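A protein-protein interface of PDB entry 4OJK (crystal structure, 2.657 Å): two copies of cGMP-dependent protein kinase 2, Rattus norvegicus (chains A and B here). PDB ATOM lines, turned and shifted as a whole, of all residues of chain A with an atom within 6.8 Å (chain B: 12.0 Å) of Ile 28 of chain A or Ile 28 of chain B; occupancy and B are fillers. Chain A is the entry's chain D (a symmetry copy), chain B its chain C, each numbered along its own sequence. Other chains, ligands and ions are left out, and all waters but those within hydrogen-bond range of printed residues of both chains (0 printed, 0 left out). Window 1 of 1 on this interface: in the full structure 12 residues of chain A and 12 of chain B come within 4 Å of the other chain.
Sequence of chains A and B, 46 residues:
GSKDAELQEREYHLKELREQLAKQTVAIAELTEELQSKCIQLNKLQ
O of Leu 21 of chain B sits close to OE1 of Gln 24 of chain A (3.3 Å).
The side-chain amide oxygen (OE1) of Gln 24 of chain B sits close to the side-chain amide oxygen (OE1) of Gln 24 of chain A (3.3 Å).
NE2 of Gln 24 of chain A sits at hydrogen-bond distance from OG1 of Thr 25 of chain B (3.1 Å).
OG1 of Thr 25 of chain B sits at hydrogen-bond distance from O of Leu 21 of chain B (2.9 Å).
The side-chain hydroxyl of Thr 32 of chain B sits at hydrogen-bond distance from the backbone carbonyl oxygen of Ile 28 of chain B (2.9 Å).
O of Ile 28 of chain A sits at hydrogen-bond distance from OG1 of Thr 32 of chain A (3.1 Å).
O of Gln 24 of chain A touches CD1 of Ile 28 of chain B (3.98 Å).
Thr 25 of chain A touches Gln 24 of chain B.
O of Gln 24 of chain B touches CD1 of Ile 28 of chain A (3.97 Å).
CG1 of Ile 28 of chain A touches CG1 of Ile 28 of chain B, 3.5 Å away.
CD1 of Leu 31 of chain B touches CG2 of Ile 28 of chain A, at 3.8 Å.
Ile 28 of chain B touches Leu 31 of chain A (CG2 to CD1, 3.8 Å).
CD1 of Leu 31 of chain B touches CB of Leu 31 of chain A, at 3.9 Å.
OG1 of Thr 32 of chain B touches CD1 of Leu 31 of chain A, 3.6 Å away.
Leu 35 of chain B touches Leu 31 of chain A.
Thr 32 of chain A touches Leu 31 of chain B.
Printed residues of chain B within 4 Å of Gln 24 of chain A: Leu 21, Gln 24, Thr 25 and Ile 28.
Of chain B, only Gln 24 comes within 4 Å of Thr 25 of chain A.
No residue of chain B comes within 4 Å of Val 26 of chain A.
No residue of chain B comes within 4 Å of Ala 27 of chain A.
Of chain B, only Gln 24, Ile 28 and Leu 31 come within 4 Å of Ile 28 of chain A.
Glu 30 of chain A touches none of the printed residues of chain B.
Of chain B, only Ile 28, Leu 31, Thr 32 and Leu 35 come within 4 Å of Leu 31 of chain A.
Thr 32 of chain A touches just one residue of chain B: Leu 31 (3.8 Å).
Of the printed residues of chain A, Leu 21 of chain B touches Gln 24 (3.3 Å).
Of the printed residues of chain A, Gln 24 of chain B touches Gln 24, Thr 25 and Ile 28.
Of chain A, only Gln 24, Ile 28 and Leu 31 come within 4 Å of Ile 28 of chain B.
Glu 30 of chain B touches none of the printed residues of chain A.
Of the printed residues of chain A, Leu 31 of chain B touches Ile 28 (3.8 Å), Leu 31 (3.9 Å) and Thr 32 (3.8 Å).
Ser 37 of chain B touches none of the printed residues of chain A.
The nearest residue of chain B that does not touch Ile 28 of chain A is Ala 27 of chain B (4.2 Å).
The nearest residue of chain A that does not touch Ile 28 of chain B is Ala 27 of chain A (4.3 Å).
The nearest printed residue of chain A that does not touch Thr 25 of chain B is Ile 28 of chain A (5.8 Å).
Of the 11 printed residues of chain A, 5 touch a printed residue of chain B.
Printed residues of chain A that touch a printed residue of chain B: Gln 24, Thr 25, Ile 28, Leu 31 and Thr 32.
Among the printed residues, 13 pairs touch across the chains.
Gln 24 of chain A touches Ile 28 of chain B, and with the chains exchanged Ile 28 of chain A touches Gln 24 of chain B.
Ile 28 of chain A touches Leu 31 of chain B, and with the chains exchanged Leu 31 of chain A touches Ile 28 of chain B.
Leu 31 of chain A touches its own counterpart, Leu 31 of chain B.
Leu 31 of chain A touches Thr 32 of chain B, and with the chains exchanged Thr 32 of chain A touches Leu 31 of chain B.
11 positions are printed for both chains.
Of the 13 pairs that touch across the chains among the printed residues, 11 have their exchanged pair printed and touching as well.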
ATOM      1  N   LYS A  23      12.464  -0.802  30.567  1.00  0.00           N
ATOM      2  CA  LYS A  23      11.253  -1.559  30.278  1.00  0.00           C
ATOM      3  C   LYS A  23      10.596  -1.097  28.980  1.00  0.00           C
ATOM      4  O   LYS A  23      10.052  -1.905  28.229  1.00  0.00           O
ATOM      5  CB  LYS A  23      10.264  -1.459  31.441  1.00  0.00           C
ATOM      6  N   GLN A  24      10.655   0.206  28.722  1.00  0.00           N
ATOM      7  CA  GLN A  24      10.052   0.776  27.518  1.00  0.00           C
ATOM      8  C   GLN A  24      10.800   0.391  26.244  1.00  0.00           C
ATOM      9  O   GLN A  24      10.182   0.178  25.200  1.00  0.00           O
ATOM     10  CB  GLN A  24       9.952   2.298  27.618  1.00  0.00           C
ATOM     11  CG  GLN A  24       8.877   2.779  28.570  1.00  0.00           C
ATOM     12  CD  GLN A  24       8.526   4.231  28.357  1.00  0.00           C
ATOM     13  OE1 GLN A  24       9.338   5.007  27.853  1.00  0.00           O
ATOM     14  NE2 GLN A  24       7.306   4.607  28.726  1.00  0.00           N
ATOM     15  N   THR A  25      12.126   0.306  26.332  1.00  0.00           N
ATOM     16  CA  THR A  25      12.937  -0.114  25.194  1.00  0.00           C
ATOM     17  C   THR A  25      12.561  -1.534  24.792  1.00  0.00           C
ATOM     18  O   THR A  25      12.383  -1.829  23.609  1.00  0.00           O
ATOM     19  CB  THR A  25      14.442  -0.055  25.511  1.00  0.00           C
ATOM     20  OG1 THR A  25      14.816   1.296  25.808  1.00  0.00           O
ATOM     21  CG2 THR A  25      15.257  -0.547  24.325  1.00  0.00           C
ATOM     22  N   VAL A  26      12.435  -2.406  25.787  1.00  0.00           N
ATOM     23  CA  VAL A  26      12.003  -3.779  25.561  1.00  0.00           C
ATOM     24  C   VAL A  26      10.643  -3.801  24.869  1.00  0.00           C
ATOM     25  O   VAL A  26      10.420  -4.577  23.938  1.00  0.00           O
ATOM     26  CB  VAL A  26      11.907  -4.554  26.887  1.00  0.00           C
ATOM     27  CG1 VAL A  26      11.492  -5.990  26.634  1.00  0.00           C
ATOM     28  CG2 VAL A  26      13.233  -4.504  27.622  1.00  0.00           C
ATOM     29  N   ALA A  27       9.740  -2.938  25.327  1.00  0.00           N
ATOM     30  CA  ALA A  27       8.408  -2.828  24.746  1.00  0.00           C
ATOM     31  C   ALA A  27       8.473  -2.378  23.292  1.00  0.00           C
ATOM     32  O   ALA A  27       7.754  -2.900  22.442  1.00  0.00           O
ATOM     33  CB  ALA A  27       7.548  -1.873  25.559  1.00  0.00           C
ATOM     34  N   ILE A  28       9.339  -1.407  23.014  1.00  0.00           N
ATOM     35  CA  ILE A  28       9.532  -0.919  21.655  1.00  0.00           C
ATOM     36  C   ILE A  28      10.085  -2.033  20.773  1.00  0.00           C
ATOM     37  O   ILE A  28       9.641  -2.217  19.639  1.00  0.00           O
ATOM     38  CB  ILE A  28      10.475   0.303  21.617  1.00  0.00           C
ATOM     39  CG1 ILE A  28       9.849   1.477  22.372  1.00  0.00           C
ATOM     40  CG2 ILE A  28      10.769   0.711  20.182  1.00  0.00           C
ATOM     41  CD1 ILE A  28      10.731   2.700  22.463  1.00  0.00           C
ATOM     42  N   ALA A  29      11.042  -2.784  21.309  1.00  0.00           N
ATOM     43  CA  ALA A  29      11.634  -3.910  20.593  1.00  0.00           C
ATOM     44  C   ALA A  29      10.588  -4.969  20.256  1.00  0.00           C
ATOM     45  O   ALA A  29      10.573  -5.502  19.148  1.00  0.00           O
ATOM     46  CB  ALA A  29      12.767  -4.519  21.406  1.00  0.00           C
ATOM     47  N   GLU A  30       9.719  -5.271  21.215  1.00  0.00           N
ATOM     48  CA  GLU A  30       8.663  -6.254  21.001  1.00  0.00           C
ATOM     49  C   GLU A  30       7.670  -5.777  19.949  1.00  0.00           C
ATOM     50  O   GLU A  30       7.282  -6.532  19.061  1.00  0.00           O
ATOM     51  CB  GLU A  30       7.933  -6.558  22.309  1.00  0.00           C
ATOM     52  CG  GLU A  30       8.773  -7.317  23.328  1.00  0.00           C
ATOM     53  CD  GLU A  30       8.003  -7.622  24.603  1.00  0.00           C
ATOM     54  OE1 GLU A  30       6.857  -7.139  24.735  1.00  0.00           O
ATOM     55  OE2 GLU A  30       8.540  -8.346  25.469  1.00  0.00           O
ATOM     56  N   LEU A  31       7.263  -4.515  20.060  1.00  0.00           N
ATOM     57  CA  LEU A  31       6.342  -3.916  19.102  1.00  0.00           C
ATOM     58  C   LEU A  31       6.909  -3.941  17.685  1.00  0.00           C
ATOM     59  O   LEU A  31       6.208  -4.288  16.736  1.00  0.00           O
ATOM     60  CB  LEU A  31       6.007  -2.481  19.511  1.00  0.00           C
ATOM     61  CG  LEU A  31       5.049  -2.339  20.692  1.00  0.00           C
ATOM     62  CD1 LEU A  31       4.928  -0.888  21.124  1.00  0.00           C
ATOM     63  CD2 LEU A  31       3.688  -2.905  20.327  1.00  0.00           C
ATOM     64  N   THR A  32       8.180  -3.567  17.556  1.00  0.00           N
ATOM     65  CA  THR A  32       8.860  -3.575  16.265  1.00  0.00           C
ATOM     66  C   THR A  32       8.864  -4.978  15.676  1.00  0.00           C
ATOM     67  O   THR A  32       8.472  -5.180  14.529  1.00  0.00           O
ATOM     68  CB  THR A  32      10.314  -3.080  16.393  1.00  0.00           C
ATOM     69  OG1 THR A  32      10.323  -1.674  16.664  1.00  0.00           O
ATOM     70  CG2 THR A  32      11.083  -3.343  15.110  1.00  0.00           C
ATOM     71  N   GLU A  33       9.301  -5.937  16.484  1.00  0.00           N
ATOM     72  CA  GLU A  33       9.386  -7.338  16.089  1.00  0.00           C
ATOM     73  C   GLU A  33       8.063  -7.849  15.532  1.00  0.00           C
ATOM     74  O   GLU A  33       8.028  -8.509  14.494  1.00  0.00           O
ATOM     75  CB  GLU A  33       9.799  -8.181  17.296  1.00  0.00           C
ATOM     76  CG  GLU A  33      10.760  -9.308  16.994  1.00  0.00           C
ATOM     77  CD  GLU A  33      11.175 -10.061  18.245  1.00  0.00           C
ATOM     78  OE1 GLU A  33      10.663  -9.727  19.336  1.00  0.00           O
ATOM     79  OE2 GLU A  33      12.013 -10.982  18.139  1.00  0.00           O
ATOM     80  N   LEU B  17      16.068  12.672  31.820  1.00  0.00           N
ATOM     81  CA  LEU B  17      15.456  11.349  31.811  1.00  0.00           C
ATOM     82  C   LEU B  17      13.998  11.395  31.366  1.00  0.00           C
ATOM     83  O   LEU B  17      13.580  10.601  30.522  1.00  0.00           O
ATOM     84  CB  LEU B  17      15.554  10.703  33.193  1.00  0.00           C
ATOM     85  CG  LEU B  17      16.875  10.007  33.520  1.00  0.00           C
ATOM     86  CD1 LEU B  17      16.801   9.344  34.888  1.00  0.00           C
ATOM     87  CD2 LEU B  17      17.219   8.988  32.444  1.00  0.00           C
ATOM     88  N   ARG B  18      13.229  12.319  31.939  1.00  0.00           N
ATOM     89  CA  ARG B  18      11.814  12.456  31.609  1.00  0.00           C
ATOM     90  C   ARG B  18      11.604  12.725  30.123  1.00  0.00           C
ATOM     91  O   ARG B  18      10.674  12.197  29.514  1.00  0.00           O
ATOM     92  CB  ARG B  18      11.161  13.565  32.440  1.00  0.00           C
ATOM     93  CG  ARG B  18      10.971  13.223  33.909  1.00  0.00           C
ATOM     94  CD  ARG B  18      10.281  14.357  34.650  1.00  0.00           C
ATOM     95  NE  ARG B  18      10.061  14.042  36.059  1.00  0.00           N
ATOM     96  N   GLU B  19      12.476  13.544  29.544  1.00  0.00           N
ATOM     97  CA  GLU B  19      12.402  13.858  28.123  1.00  0.00           C
ATOM     98  C   GLU B  19      12.581  12.591  27.294  1.00  0.00           C
ATOM     99  O   GLU B  19      11.865  12.375  26.316  1.00  0.00           O
ATOM    100  CB  GLU B  19      13.457  14.899  27.747  1.00  0.00           C
ATOM    101  CG  GLU B  19      13.326  15.440  26.331  1.00  0.00           C
ATOM    102  CD  GLU B  19      14.320  16.549  26.033  1.00  0.00           C
ATOM    103  OE1 GLU B  19      14.388  16.987  24.866  1.00  0.00           O
ATOM    104  OE2 GLU B  19      15.031  16.985  26.964  1.00  0.00           O
ATOM    105  N   GLN B  20      13.530  11.752  27.703  1.00  0.00           N
ATOM    106  CA  GLN B  20      13.772  10.470  27.045  1.00  0.00           C
ATOM    107  C   GLN B  20      12.580   9.539  27.229  1.00  0.00           C
ATOM    108  O   GLN B  20      12.159   8.851  26.300  1.00  0.00           O
ATOM    109  CB  GLN B  20      15.023   9.808  27.624  1.00  0.00           C
ATOM    110  CG  GLN B  20      16.199   9.718  26.662  1.00  0.00           C
ATOM    111  CD  GLN B  20      16.053   8.600  25.644  1.00  0.00           C
ATOM    112  OE1 GLN B  20      15.130   8.599  24.830  1.00  0.00           O
ATOM    113  NE2 GLN B  20      16.968   7.637  25.689  1.00  0.00           N
ATOM    114  N   LEU B  21      12.050   9.528  28.446  1.00  0.00           N
ATOM    115  CA  LEU B  21      10.897   8.709  28.795  1.00  0.00           C
ATOM    116  C   LEU B  21       9.706   9.129  27.948  1.00  0.00           C
ATOM    117  O   LEU B  21       8.987   8.293  27.417  1.00  0.00           O
ATOM    118  CB  LEU B  21      10.575   8.867  30.286  1.00  0.00           C
ATOM    119  CG  LEU B  21      10.301   7.613  31.119  1.00  0.00           C
ATOM    120  CD1 LEU B  21       9.089   6.856  30.598  1.00  0.00           C
ATOM    121  CD2 LEU B  21      11.529   6.718  31.163  1.00  0.00           C
ATOM    122  N   ALA B  22       9.515  10.438  27.830  1.00  0.00           N
ATOM    123  CA  ALA B  22       8.421  10.999  27.052  1.00  0.00           C
ATOM    124  C   ALA B  22       8.524  10.600  25.582  1.00  0.00           C
ATOM    125  O   ALA B  22       7.536  10.192  24.969  1.00  0.00           O
ATOM    126  CB  ALA B  22       8.396  12.512  27.192  1.00  0.00           C
ATOM    127  N   LYS B  23       9.718  10.731  25.015  1.00  0.00           N
ATOM    128  CA  LYS B  23       9.917  10.458  23.595  1.00  0.00           C
ATOM    129  C   LYS B  23       9.733   8.982  23.249  1.00  0.00           C
ATOM    130  O   LYS B  23       9.198   8.653  22.194  1.00  0.00           O
ATOM    131  CB  LYS B  23      11.278  10.978  23.128  1.00  0.00           C
ATOM    132  CG  LYS B  23      11.335  12.497  23.024  1.00  0.00           C
ATOM    133  CD  LYS B  23      12.726  12.995  22.665  1.00  0.00           C
ATOM    134  CE  LYS B  23      12.745  14.508  22.549  1.00  0.00           C
ATOM    135  NZ  LYS B  23      14.092  15.015  22.183  1.00  0.00           N
ATOM    136  N   GLN B  24      10.163   8.098  24.144  1.00  0.00           N
ATOM    137  CA  GLN B  24       9.942   6.669  23.960  1.00  0.00           C
ATOM    138  C   GLN B  24       8.457   6.320  24.014  1.00  0.00           C
ATOM    139  O   GLN B  24       7.987   5.458  23.275  1.00  0.00           O
ATOM    140  CB  GLN B  24      10.716   5.860  25.003  1.00  0.00           C
ATOM    141  CG  GLN B  24      12.224   5.894  24.813  1.00  0.00           C
ATOM    142  CD  GLN B  24      12.957   4.961  25.759  1.00  0.00           C
ATOM    143  OE1 GLN B  24      12.372   4.420  26.699  1.00  0.00           O
ATOM    144  NE2 GLN B  24      14.248   4.765  25.509  1.00  0.00           N
ATOM    145  N   THR B  25       7.724   6.999  24.889  1.00  0.00           N
ATOM    146  CA  THR B  25       6.280   6.807  25.000  1.00  0.00           C
ATOM    147  C   THR B  25       5.580   7.191  23.700  1.00  0.00           C
ATOM    148  O   THR B  25       4.659   6.509  23.256  1.00  0.00           O
ATOM    149  CB  THR B  25       5.692   7.633  26.157  1.00  0.00           C
ATOM    150  OG1 THR B  25       6.326   7.246  27.380  1.00  0.00           O
ATOM    151  CG2 THR B  25       4.199   7.408  26.275  1.00  0.00           C
ATOM    152  N   VAL B  26       6.031   8.281  23.090  1.00  0.00           N
ATOM    153  CA  VAL B  26       5.501   8.707  21.801  1.00  0.00           C
ATOM    154  C   VAL B  26       5.782   7.650  20.740  1.00  0.00           C
ATOM    155  O   VAL B  26       4.929   7.363  19.894  1.00  0.00           O
ATOM    156  CB  VAL B  26       6.118  10.042  21.361  1.00  0.00           C
ATOM    157  CG1 VAL B  26       5.595  10.447  19.994  1.00  0.00           C
ATOM    158  CG2 VAL B  26       5.817  11.113  22.381  1.00  0.00           C
ATOM    159  N   ALA B  27       6.978   7.069  20.800  1.00  0.00           N
ATOM    160  CA  ALA B  27       7.371   6.012  19.878  1.00  0.00           C
ATOM    161  C   ALA B  27       6.455   4.804  20.021  1.00  0.00           C
ATOM    162  O   ALA B  27       5.961   4.267  19.028  1.00  0.00           O
ATOM    163  CB  ALA B  27       8.815   5.610  20.121  1.00  0.00           C
ATOM    164  N   ILE B  28       6.234   4.388  21.264  1.00  0.00           N
ATOM    165  CA  ILE B  28       5.381   3.243  21.561  1.00  0.00           C
ATOM    166  C   ILE B  28       3.969   3.432  21.015  1.00  0.00           C
ATOM    167  O   ILE B  28       3.411   2.528  20.395  1.00  0.00           O
ATOM    168  CB  ILE B  28       5.331   2.971  23.077  1.00  0.00           C
ATOM    169  CG1 ILE B  28       6.680   2.426  23.548  1.00  0.00           C
ATOM    170  CG2 ILE B  28       4.221   1.996  23.415  1.00  0.00           C
ATOM    171  CD1 ILE B  28       6.812   2.287  25.042  1.00  0.00           C
ATOM    172  N   ALA B  29       3.406   4.617  21.231  1.00  0.00           N
ATOM    173  CA  ALA B  29       2.056   4.919  20.765  1.00  0.00           C
ATOM    174  C   ALA B  29       1.952   4.857  19.241  1.00  0.00           C
ATOM    175  O   ALA B  29       0.945   4.398  18.699  1.00  0.00           O
ATOM    176  CB  ALA B  29       1.604   6.276  21.280  1.00  0.00           C
ATOM    177  N   GLU B  30       2.996   5.314  18.557  1.00  0.00           N
ATOM    178  CA  GLU B  30       3.004   5.306  17.097  1.00  0.00           C
ATOM    179  C   GLU B  30       3.099   3.883  16.556  1.00  0.00           C
ATOM    180  O   GLU B  30       2.434   3.537  15.584  1.00  0.00           O
ATOM    181  CB  GLU B  30       4.151   6.158  16.552  1.00  0.00           C
ATOM    182  CG  GLU B  30       4.240   6.169  15.032  1.00  0.00           C
ATOM    183  CD  GLU B  30       5.308   7.111  14.512  1.00  0.00           C
ATOM    184  OE1 GLU B  30       5.652   7.018  13.314  1.00  0.00           O
ATOM    185  OE2 GLU B  30       5.800   7.949  15.297  1.00  0.00           O
ATOM    186  N   LEU B  31       3.927   3.062  17.195  1.00  0.00           N
ATOM    187  CA  LEU B  31       4.079   1.670  16.796  1.00  0.00           C
ATOM    188  C   LEU B  31       2.796   0.885  17.029  1.00  0.00           C
ATOM    189  O   LEU B  31       2.365   0.114  16.170  1.00  0.00           O
ATOM    190  CB  LEU B  31       5.235   1.019  17.558  1.00  0.00           C
ATOM    191  CG  LEU B  31       6.637   1.395  17.083  1.00  0.00           C
ATOM    192  CD1 LEU B  31       7.697   0.694  17.920  1.00  0.00           C
ATOM    193  CD2 LEU B  31       6.796   1.049  15.616  1.00  0.00           C
ATOM    194  N   THR B  32       2.187   1.086  18.193  1.00  0.00           N
ATOM    195  CA  THR B  32       0.969   0.374  18.549  1.00  0.00           C
ATOM    196  C   THR B  32      -0.161   0.686  17.572  1.00  0.00           C
ATOM    197  O   THR B  32      -0.892  -0.210  17.153  1.00  0.00           O
ATOM    198  CB  THR B  32       0.521   0.704  19.987  1.00  0.00           C
ATOM    199  OG1 THR B  32       1.558   0.344  20.910  1.00  0.00           O
ATOM    200  CG2 THR B  32      -0.752  -0.057  20.340  1.00  0.00           C
ATOM    201  N   GLU B  33      -0.290   1.955  17.201  1.00  0.00           N
ATOM    202  CA  GLU B  33      -1.340   2.371  16.282  1.00  0.00           C
ATOM    203  C   GLU B  33      -1.163   1.701  14.928  1.00  0.00           C
ATOM    204  O   GLU B  33      -2.129   1.231  14.330  1.00  0.00           O
ATOM    205  CB  GLU B  33      -1.356   3.892  16.122  1.00  0.00           C
ATOM    206  CG  GLU B  33      -2.520   4.406  15.294  1.00  0.00           C
ATOM    207  CD  GLU B  33      -2.514   5.912  15.138  1.00  0.00           C
ATOM    208  OE1 GLU B  33      -3.603   6.521  15.213  1.00  0.00           O
ATOM    209  OE2 GLU B  33      -1.426   6.486  14.934  1.00  0.00           O
ATOM    210  N   GLU B  34       0.080   1.661  14.455  1.00  0.00           N
ATOM    211  CA  GLU B  34       0.407   1.008  13.196  1.00  0.00           C
ATOM    212  C   GLU B  34       0.143  -0.490  13.290  1.00  0.00           C
ATOM    213  O   GLU B  34      -0.352  -1.098  12.345  1.00  0.00           O
ATOM    214  CB  GLU B  34       1.870   1.264  12.821  1.00  0.00           C
ATOM    215  CG  GLU B  34       2.187   2.714  12.466  1.00  0.00           C
ATOM    216  CD  GLU B  34       3.640   2.923  12.069  1.00  0.00           C
ATOM    217  OE1 GLU B  34       4.388   1.926  12.003  1.00  0.00           O
ATOM    218  OE2 GLU B  34       4.036   4.083  11.822  1.00  0.00           O
ATOM    219  N   LEU B  35       0.470  -1.075  14.438  1.00  0.00           N
ATOM    220  CA  LEU B  35       0.281  -2.507  14.653  1.00  0.00           C
ATOM    221  C   LEU B  35      -1.203  -2.862  14.731  1.00  0.00           C
ATOM    222  O   LEU B  35      -1.616  -3.929  14.270  1.00  0.00           O
ATOM    223  CB  LEU B  35       1.035  -2.960  15.904  1.00  0.00           C
ATOM    224  CG  LEU B  35       1.152  -4.457  16.185  1.00  0.00           C
ATOM    225  CD1 LEU B  35       1.414  -5.240  14.910  1.00  0.00           C
ATOM    226  CD2 LEU B  35       2.262  -4.707  17.197  1.00  0.00           C
ATOM    227  N   GLN B  36      -1.998  -1.958  15.301  1.00  0.00           N
ATOM    228  CA  GLN B  36      -3.450  -2.102  15.292  1.00  0.00           C
ATOM    229  C   GLN B  36      -3.966  -2.189  13.864  1.00  0.00           C
ATOM    230  O   GLN B  36      -4.698  -3.112  13.512  1.00  0.00           O
ATOM    231  CB  GLN B  36      -4.126  -0.911  15.973  1.00  0.00           C
ATOM    232  CG  GLN B  36      -4.123  -0.954  17.488  1.00  0.00           C
ATOM    233  CD  GLN B  36      -5.291  -0.191  18.084  1.00  0.00           C
ATOM    234  OE1 GLN B  36      -5.694  -0.439  19.218  1.00  0.00           O
ATOM    235  NE2 GLN B  36      -5.841   0.742  17.316  1.00  0.00           N
ATOM    236  N   SER B  37      -3.577  -1.214  13.047  1.00  0.00           N
ATOM    237  CA  SER B  37      -4.044  -1.128  11.671  1.00  0.00           C
ATOM    238  C   SER B  37      -3.627  -2.348  10.856  1.00  0.00           C
ATOM    239  O   SER B  37      -4.371  -2.808   9.993  1.00  0.00           O
ATOM    240  CB  SER B  37      -3.528   0.152  11.012  1.00  0.00           C
ATOM    241  OG  SER B  37      -4.057   0.294   9.705  1.00  0.00           O
